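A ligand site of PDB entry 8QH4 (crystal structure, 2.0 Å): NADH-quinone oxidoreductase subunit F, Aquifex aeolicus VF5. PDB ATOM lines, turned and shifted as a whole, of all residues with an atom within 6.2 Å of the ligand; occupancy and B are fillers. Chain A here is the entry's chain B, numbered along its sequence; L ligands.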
ATOM      1  N   ILE A 181     -16.532  -2.258 -14.910  1.00  0.00           N
ATOM      2  CA  ILE A 181     -16.175  -3.611 -15.280  1.00  0.00           C
ATOM      3  C   ILE A 181     -14.818  -3.637 -15.980  1.00  0.00           C
ATOM      4  O   ILE A 181     -14.227  -4.700 -16.102  1.00  0.00           O
ATOM      5  CB  ILE A 181     -17.271  -4.269 -16.161  1.00  0.00           C
ATOM      6  CG1 ILE A 181     -17.101  -5.788 -16.254  1.00  0.00           C
ATOM      7  CG2 ILE A 181     -17.328  -3.629 -17.548  1.00  0.00           C
ATOM      8  CD1 ILE A 181     -17.161  -6.501 -14.925  1.00  0.00           C
ATOM      9  N   HIS A 198     -16.017  -6.386 -22.150  1.00  0.00           N
ATOM     10  CA  HIS A 198     -16.704  -7.631 -21.858  1.00  0.00           C
ATOM     11  C   HIS A 198     -15.702  -8.640 -21.303  1.00  0.00           C
ATOM     12  O   HIS A 198     -14.745  -9.011 -22.001  1.00  0.00           O
ATOM     13  CB  HIS A 198     -17.383  -8.177 -23.107  1.00  0.00           C
ATOM     14  CG  HIS A 198     -18.590  -7.406 -23.514  1.00  0.00           C
ATOM     15  ND1 HIS A 198     -19.123  -7.497 -24.778  1.00  0.00           N
ATOM     16  CD2 HIS A 198     -19.363  -6.531 -22.865  1.00  0.00           C
ATOM     17  CE1 HIS A 198     -20.191  -6.718 -24.857  1.00  0.00           C
ATOM     18  NE2 HIS A 198     -20.368  -6.132 -23.709  1.00  0.00           N
ATOM     19  N   PRO A 199     -15.836  -9.086 -20.030  1.00  0.00           N
ATOM     20  CA  PRO A 199     -14.946 -10.110 -19.489  1.00  0.00           C
ATOM     21  C   PRO A 199     -14.922 -11.396 -20.327  1.00  0.00           C
ATOM     22  O   PRO A 199     -15.928 -11.752 -20.943  1.00  0.00           O
ATOM     23  CB  PRO A 199     -15.516 -10.389 -18.085  1.00  0.00           C
ATOM     24  CG  PRO A 199     -16.198  -9.070 -17.712  1.00  0.00           C
ATOM     25  CD  PRO A 199     -16.754  -8.532 -19.020  1.00  0.00           C
ATOM     26  N   GLU A 345     -23.442  -1.202 -13.499  1.00  0.00           N
ATOM     27  CA  GLU A 345     -22.119  -1.659 -13.928  1.00  0.00           C
ATOM     28  C   GLU A 345     -22.087  -3.077 -14.514  1.00  0.00           C
ATOM     29  O   GLU A 345     -21.070  -3.457 -15.089  1.00  0.00           O
ATOM     30  CB  GLU A 345     -21.119  -1.535 -12.773  1.00  0.00           C
ATOM     31  CG  GLU A 345     -20.948  -0.104 -12.280  1.00  0.00           C
ATOM     32  CD  GLU A 345     -20.570   0.911 -13.339  1.00  0.00           C
ATOM     33  OE1 GLU A 345     -19.982   0.507 -14.386  1.00  0.00           O
ATOM     34  OE2 GLU A 345     -20.875   2.107 -13.137  1.00  0.00           O
ATOM     35  N   THR A 346     -23.155  -3.879 -14.392  1.00  0.00           N
ATOM     36  CA  THR A 346     -23.166  -5.154 -15.097  1.00  0.00           C
ATOM     37  C   THR A 346     -23.018  -4.918 -16.598  1.00  0.00           C
ATOM     38  O   THR A 346     -23.690  -4.042 -17.164  1.00  0.00           O
ATOM     39  CB  THR A 346     -24.438  -5.968 -14.829  1.00  0.00           C
ATOM     40  OG1 THR A 346     -24.420  -7.067 -15.737  1.00  0.00           O
ATOM     41  CG2 THR A 346     -25.724  -5.190 -14.985  1.00  0.00           C
ATOM     42  N   CYS A 347     -22.168  -5.721 -17.261  1.00  0.00           N
ATOM     43  CA  CYS A 347     -21.944  -5.580 -18.695  1.00  0.00           C
ATOM     44  C   CYS A 347     -23.047  -6.288 -19.502  1.00  0.00           C
ATOM     45  O   CYS A 347     -23.190  -6.034 -20.694  1.00  0.00           O
ATOM     46  CB  CYS A 347     -20.553  -6.084 -19.073  1.00  0.00           C
ATOM     47  SG  CYS A 347     -20.396  -7.875 -19.261  1.00  0.00           S
ATOM     48  N   GLY A 348     -23.812  -7.183 -18.868  1.00  0.00           N
ATOM     49  CA  GLY A 348     -25.000  -7.749 -19.498  1.00  0.00           C
ATOM     50  C   GLY A 348     -24.759  -9.019 -20.306  1.00  0.00           C
ATOM     51  O   GLY A 348     -25.720  -9.592 -20.819  1.00  0.00           O
ATOM     52  N   GLN A 349     -23.513  -9.505 -20.411  1.00  0.00           N
ATOM     53  CA  GLN A 349     -23.239 -10.714 -21.182  1.00  0.00           C
ATOM     54  C   GLN A 349     -24.006 -11.913 -20.604  1.00  0.00           C
ATOM     55  O   GLN A 349     -24.484 -12.760 -21.363  1.00  0.00           O
ATOM     56  CB  GLN A 349     -21.756 -11.082 -21.142  1.00  0.00           C
ATOM     57  CG  GLN A 349     -20.844 -10.274 -22.040  1.00  0.00           C
ATOM     58  CD  GLN A 349     -19.495 -10.954 -22.033  1.00  0.00           C
ATOM     59  OE1 GLN A 349     -19.226 -11.791 -22.899  1.00  0.00           O
ATOM     60  NE2 GLN A 349     -18.704 -10.691 -20.993  1.00  0.00           N
ATOM     61  N   CYS A 350     -24.047 -12.001 -19.271  1.00  0.00           N
ATOM     62  CA  CYS A 350     -24.646 -13.144 -18.587  1.00  0.00           C
ATOM     63  C   CYS A 350     -26.071 -12.773 -18.154  1.00  0.00           C
ATOM     64  O   CYS A 350     -26.294 -11.677 -17.630  1.00  0.00           O
ATOM     65  CB  CYS A 350     -23.805 -13.600 -17.392  1.00  0.00           C
ATOM     66  SG  CYS A 350     -22.002 -13.593 -17.668  1.00  0.00           S
ATOM     67  N   THR A 351     -27.014 -13.698 -18.338  1.00  0.00           N
ATOM     68  CA  THR A 351     -28.429 -13.407 -18.162  1.00  0.00           C
ATOM     69  C   THR A 351     -28.741 -13.174 -16.683  1.00  0.00           C
ATOM     70  O   THR A 351     -29.399 -12.186 -16.358  1.00  0.00           O
ATOM     71  CB  THR A 351     -29.291 -14.485 -18.837  1.00  0.00           C
ATOM     72  OG1 THR A 351     -29.228 -14.285 -20.250  1.00  0.00           O
ATOM     73  CG2 THR A 351     -30.731 -14.456 -18.383  1.00  0.00           C
ATOM     74  N   CYS A 353     -26.843 -12.270 -14.193  1.00  0.00           N
ATOM     75  CA  CYS A 353     -26.223 -11.004 -13.833  1.00  0.00           C
ATOM     76  C   CYS A 353     -27.008  -9.823 -14.423  1.00  0.00           C
ATOM     77  O   CYS A 353     -27.345  -8.883 -13.705  1.00  0.00           O
ATOM     78  CB  CYS A 353     -24.768 -10.937 -14.281  1.00  0.00           C
ATOM     79  SG  CYS A 353     -23.896  -9.465 -13.658  1.00  0.00           S
ATOM     80  N   ARG A 354     -27.304  -9.892 -15.728  1.00  0.00           N
ATOM     81  CA  ARG A 354     -27.958  -8.804 -16.442  1.00  0.00           C
ATOM     82  C   ARG A 354     -29.301  -8.477 -15.784  1.00  0.00           C
ATOM     83  O   ARG A 354     -29.532  -7.345 -15.366  1.00  0.00           O
ATOM     84  CB  ARG A 354     -28.137  -9.176 -17.914  1.00  0.00           C
ATOM     85  CG  ARG A 354     -28.993  -8.205 -18.718  1.00  0.00           C
ATOM     86  CD  ARG A 354     -29.050  -8.561 -20.197  1.00  0.00           C
ATOM     87  NE  ARG A 354     -29.859  -9.741 -20.489  1.00  0.00           N
ATOM     88  CZ  ARG A 354     -29.371 -10.911 -20.915  1.00  0.00           C
ATOM     89  NH1 ARG A 354     -30.202 -11.896 -21.226  1.00  0.00           N
ATOM     90  NH2 ARG A 354     -28.068 -11.088 -21.033  1.00  0.00           N
ATOM     91  N   CYS A 357     -28.990  -7.916 -11.531  1.00  0.00           N
ATOM     92  CA  CYS A 357     -28.508  -6.633 -11.044  1.00  0.00           C
ATOM     93  C   CYS A 357     -29.604  -5.570 -11.190  1.00  0.00           C
ATOM     94  O   CYS A 357     -29.840  -4.770 -10.266  1.00  0.00           O
ATOM     95  CB  CYS A 357     -27.206  -6.217 -11.721  1.00  0.00           C
ATOM     96  SG  CYS A 357     -25.792  -7.206 -11.149  1.00  0.00           S
ATOM     97  N   ILE A 387     -28.108 -14.016  -8.657  1.00  0.00           N
ATOM     98  CA  ILE A 387     -27.387 -13.186  -9.610  1.00  0.00           C
ATOM     99  C   ILE A 387     -26.181 -13.958 -10.154  1.00  0.00           C
ATOM    100  O   ILE A 387     -25.828 -13.799 -11.328  1.00  0.00           O
ATOM    101  CB  ILE A 387     -26.968 -11.837  -8.972  1.00  0.00           C
ATOM    102  CG1 ILE A 387     -28.177 -11.052  -8.463  1.00  0.00           C
ATOM    103  CG2 ILE A 387     -26.138 -11.029  -9.963  1.00  0.00           C
ATOM    104  CD1 ILE A 387     -27.835  -9.803  -7.672  1.00  0.00           C
ATOM    105  N   THR A 390     -24.172 -18.941 -13.713  1.00  0.00           N
ATOM    106  CA  THR A 390     -23.648 -18.862 -15.081  1.00  0.00           C
ATOM    107  C   THR A 390     -22.691 -17.678 -15.277  1.00  0.00           C
ATOM    108  O   THR A 390     -22.149 -17.521 -16.367  1.00  0.00           O
ATOM    109  CB  THR A 390     -24.745 -18.814 -16.152  1.00  0.00           C
ATOM    110  OG1 THR A 390     -25.282 -17.494 -16.253  1.00  0.00           O
ATOM    111  CG2 THR A 390     -25.871 -19.800 -15.914  1.00  0.00           C
ATOM    112  N   SER A 391     -22.469 -16.864 -14.240  1.00  0.00           N
ATOM    113  CA  SER A 391     -21.662 -15.660 -14.388  1.00  0.00           C
ATOM    114  C   SER A 391     -20.226 -16.008 -14.795  1.00  0.00           C
ATOM    115  O   SER A 391     -19.648 -16.988 -14.321  1.00  0.00           O
ATOM    116  CB  SER A 391     -21.683 -14.825 -13.144  1.00  0.00           C
ATOM    117  OG  SER A 391     -21.181 -15.554 -12.030  1.00  0.00           O
ATOM    118  N   ILE A 392     -19.641 -15.194 -15.684  1.00  0.00           N
ATOM    119  CA  ILE A 392     -18.284 -15.488 -16.126  1.00  0.00           C
ATOM    120  C   ILE A 392     -17.259 -14.612 -15.425  1.00  0.00           C
ATOM    121  O   ILE A 392     -16.071 -14.838 -15.638  1.00  0.00           O
ATOM    122  CB  ILE A 392     -18.135 -15.470 -17.669  1.00  0.00           C
ATOM    123  CG1 ILE A 392     -18.467 -14.126 -18.321  1.00  0.00           C
ATOM    124  CG2 ILE A 392     -18.948 -16.592 -18.283  1.00  0.00           C
ATOM    125  CD1 ILE A 392     -18.609 -14.216 -19.836  1.00  0.00           C
ATOM    126  N   CYS A 393     -17.672 -13.625 -14.613  1.00  0.00           N
ATOM    127  CA  CYS A 393     -16.711 -12.808 -13.865  1.00  0.00           C
ATOM    128  C   CYS A 393     -17.208 -12.555 -12.448  1.00  0.00           C
ATOM    129  O   CYS A 393     -18.305 -12.980 -12.070  1.00  0.00           O
ATOM    130  CB  CYS A 393     -16.343 -11.502 -14.569  1.00  0.00           C
ATOM    131  SG  CYS A 393     -17.390 -10.065 -14.175  1.00  0.00           S
ATOM    132  N   GLY A 394     -16.348 -11.907 -11.670  1.00  0.00           N
ATOM    133  CA  GLY A 394     -16.534 -11.737 -10.238  1.00  0.00           C
ATOM    134  C   GLY A 394     -17.691 -10.814  -9.854  1.00  0.00           C
ATOM    135  O   GLY A 394     -18.194 -10.897  -8.728  1.00  0.00           O
ATOM    136  N   LEU A 395     -18.108  -9.939 -10.779  1.00  0.00           N
ATOM    137  CA  LEU A 395     -19.190  -8.994 -10.497  1.00  0.00           C
ATOM    138  C   LEU A 395     -20.500  -9.742 -10.211  1.00  0.00           C
ATOM    139  O   LEU A 395     -21.160  -9.476  -9.207  1.00  0.00           O
ATOM    140  CB  LEU A 395     -19.325  -8.014 -11.662  1.00  0.00           C
ATOM    141  CG  LEU A 395     -20.258  -6.834 -11.407  1.00  0.00           C
ATOM    142  CD1 LEU A 395     -19.874  -5.627 -12.254  1.00  0.00           C
ATOM    143  CD2 LEU A 395     -21.711  -7.232 -11.686  1.00  0.00           C
ATOM    144  N   GLY A 396     -20.854 -10.693 -11.092  1.00  0.00           N
ATOM    145  CA  GLY A 396     -22.047 -11.505 -10.886  1.00  0.00           C
ATOM    146  C   GLY A 396     -21.951 -12.353  -9.626  1.00  0.00           C
ATOM    147  O   GLY A 396     -22.939 -12.563  -8.937  1.00  0.00           O
ATOM    148  N   ALA A 397     -20.727 -12.782  -9.294  1.00  0.00           N
ATOM    149  CA  ALA A 397     -20.485 -13.597  -8.113  1.00  0.00           C
ATOM    150  C   ALA A 397     -20.788 -12.824  -6.815  1.00  0.00           C
ATOM    151  O   ALA A 397     -21.153 -13.466  -5.836  1.00  0.00           O
ATOM    152  CB  ALA A 397     -19.073 -14.136  -8.127  1.00  0.00           C
HETATM  153 FE1  LIG L   1     -20.749  -9.048 -17.358  1.00  0.00          FE
HETATM  154 FE2  LIG L   1     -22.040  -9.728 -14.996  1.00  0.00          FE
HETATM  155 FE3  LIG L   1     -19.357 -10.269 -15.309  1.00  0.00          FE
HETATM  156 FE4  LIG L   1     -21.240 -11.686 -16.746  1.00  0.00          FE
HETATM  157  S1  LIG L   1     -20.935 -11.695 -14.429  1.00  0.00           S
HETATM  158  S2  LIG L   1     -19.278 -10.851 -17.558  1.00  0.00           S
HETATM  159  S3  LIG L   1     -22.815 -10.026 -17.164  1.00  0.00           S
HETATM  160  S4  LIG L   1     -20.383  -8.181 -15.281  1.00  0.00           S
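The side-chain sulfur (SG) of Cys 350 lies close to the backbone NH (N) of Ile 392 (3.5 Å). The side-chain sulfur (SG) of Cys 347 lies close to the backbone NH (N) of Gln 349 (3.7 Å). N of Leu 395 sits close to SG of Cys 393, at 3.5 Å. The backbone carbonyl oxygen (O) of Cys 353 sits close to the side-chain sulfur (SG) of Cys 357 (3.4 Å). The backbone carbonyl oxygen (O) of Ile 387 sits at hydrogen-bond distance from the backbone NH (N) of Cys 353 (3.4 Å). The side-chain amide nitrogen of Gln 349 lies within hydrogen-bond range of the backbone carbonyl oxygen of Pro 199, at 3.0 Å. The backbone NH (N) of Gly 348 is in hydrogen-bond range of the side-chain hydroxyl (OG1) of Thr 346, 3.2 Å away. NH2 of Arg 354 lies within hydrogen-bond range of O of Gly 348, at 2.8 Å.
Residues that only touch the ligand: Ile 181 (3.7 Å), Pro 199 (3.6 Å), Ser 391 (3.5 Å), Ile 392 (3.5 Å) and Leu 395 (3.8 Å). Hydrophobic or aromatic side chains within 4 Å of the ligand: Ile 181, Pro 199, Ile 392 and Leu 395. 13 residues have an atom within 4 Å of the ligand: Ile 181, Pro 199, Thr 346, Cys 347, Gly 348, Gln 349, Cys 350, Cys 353, Ser 391, Ile 392, Cys 393, Leu 395 and Gly 396. Along chain A the residues within 4 Å of the ligand span positions 181 to 396. The nearest printed residue that does not touch the ligand is Arg 354 (4.7 Å).
N of Cys 350 sits close to S3 of the ligand (3.1 Å). The side-chain sulfur (SG) of Cys 350 binds an iron atom (FE4) of the ligand (2.3 Å). The backbone NH (N) of Cys 347 sits close to a sulfur (S4) of the ligand (3.6 Å). SG of Cys 347 is bound to FE1 of the ligand (2.3 Å). N of Cys 393 sits close to S1 of the ligand (3.8 Å). The side-chain sulfur (SG) of Cys 393 binds an iron atom (FE3) of the ligand. An iron atom (FE2) of the ligand is bound by the side-chain sulfur of Cys 353, 2.3 Å away. A sulfur (S3) of the ligand lies close to the backbone NH (N) of Gln 349 (3.4 Å). NE2 of Gln 349 lies close to S2 of the ligand. The backbone NH (N) of Gly 348 lies close to a sulfur (S3) of the ligand (3.5 Å). The backbone NH of Gly 396 sits close to a sulfur (S1) of the ligand (3.5 Å). S3 of the ligand sits close to OG1 of Thr 346 (3.7 Å).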
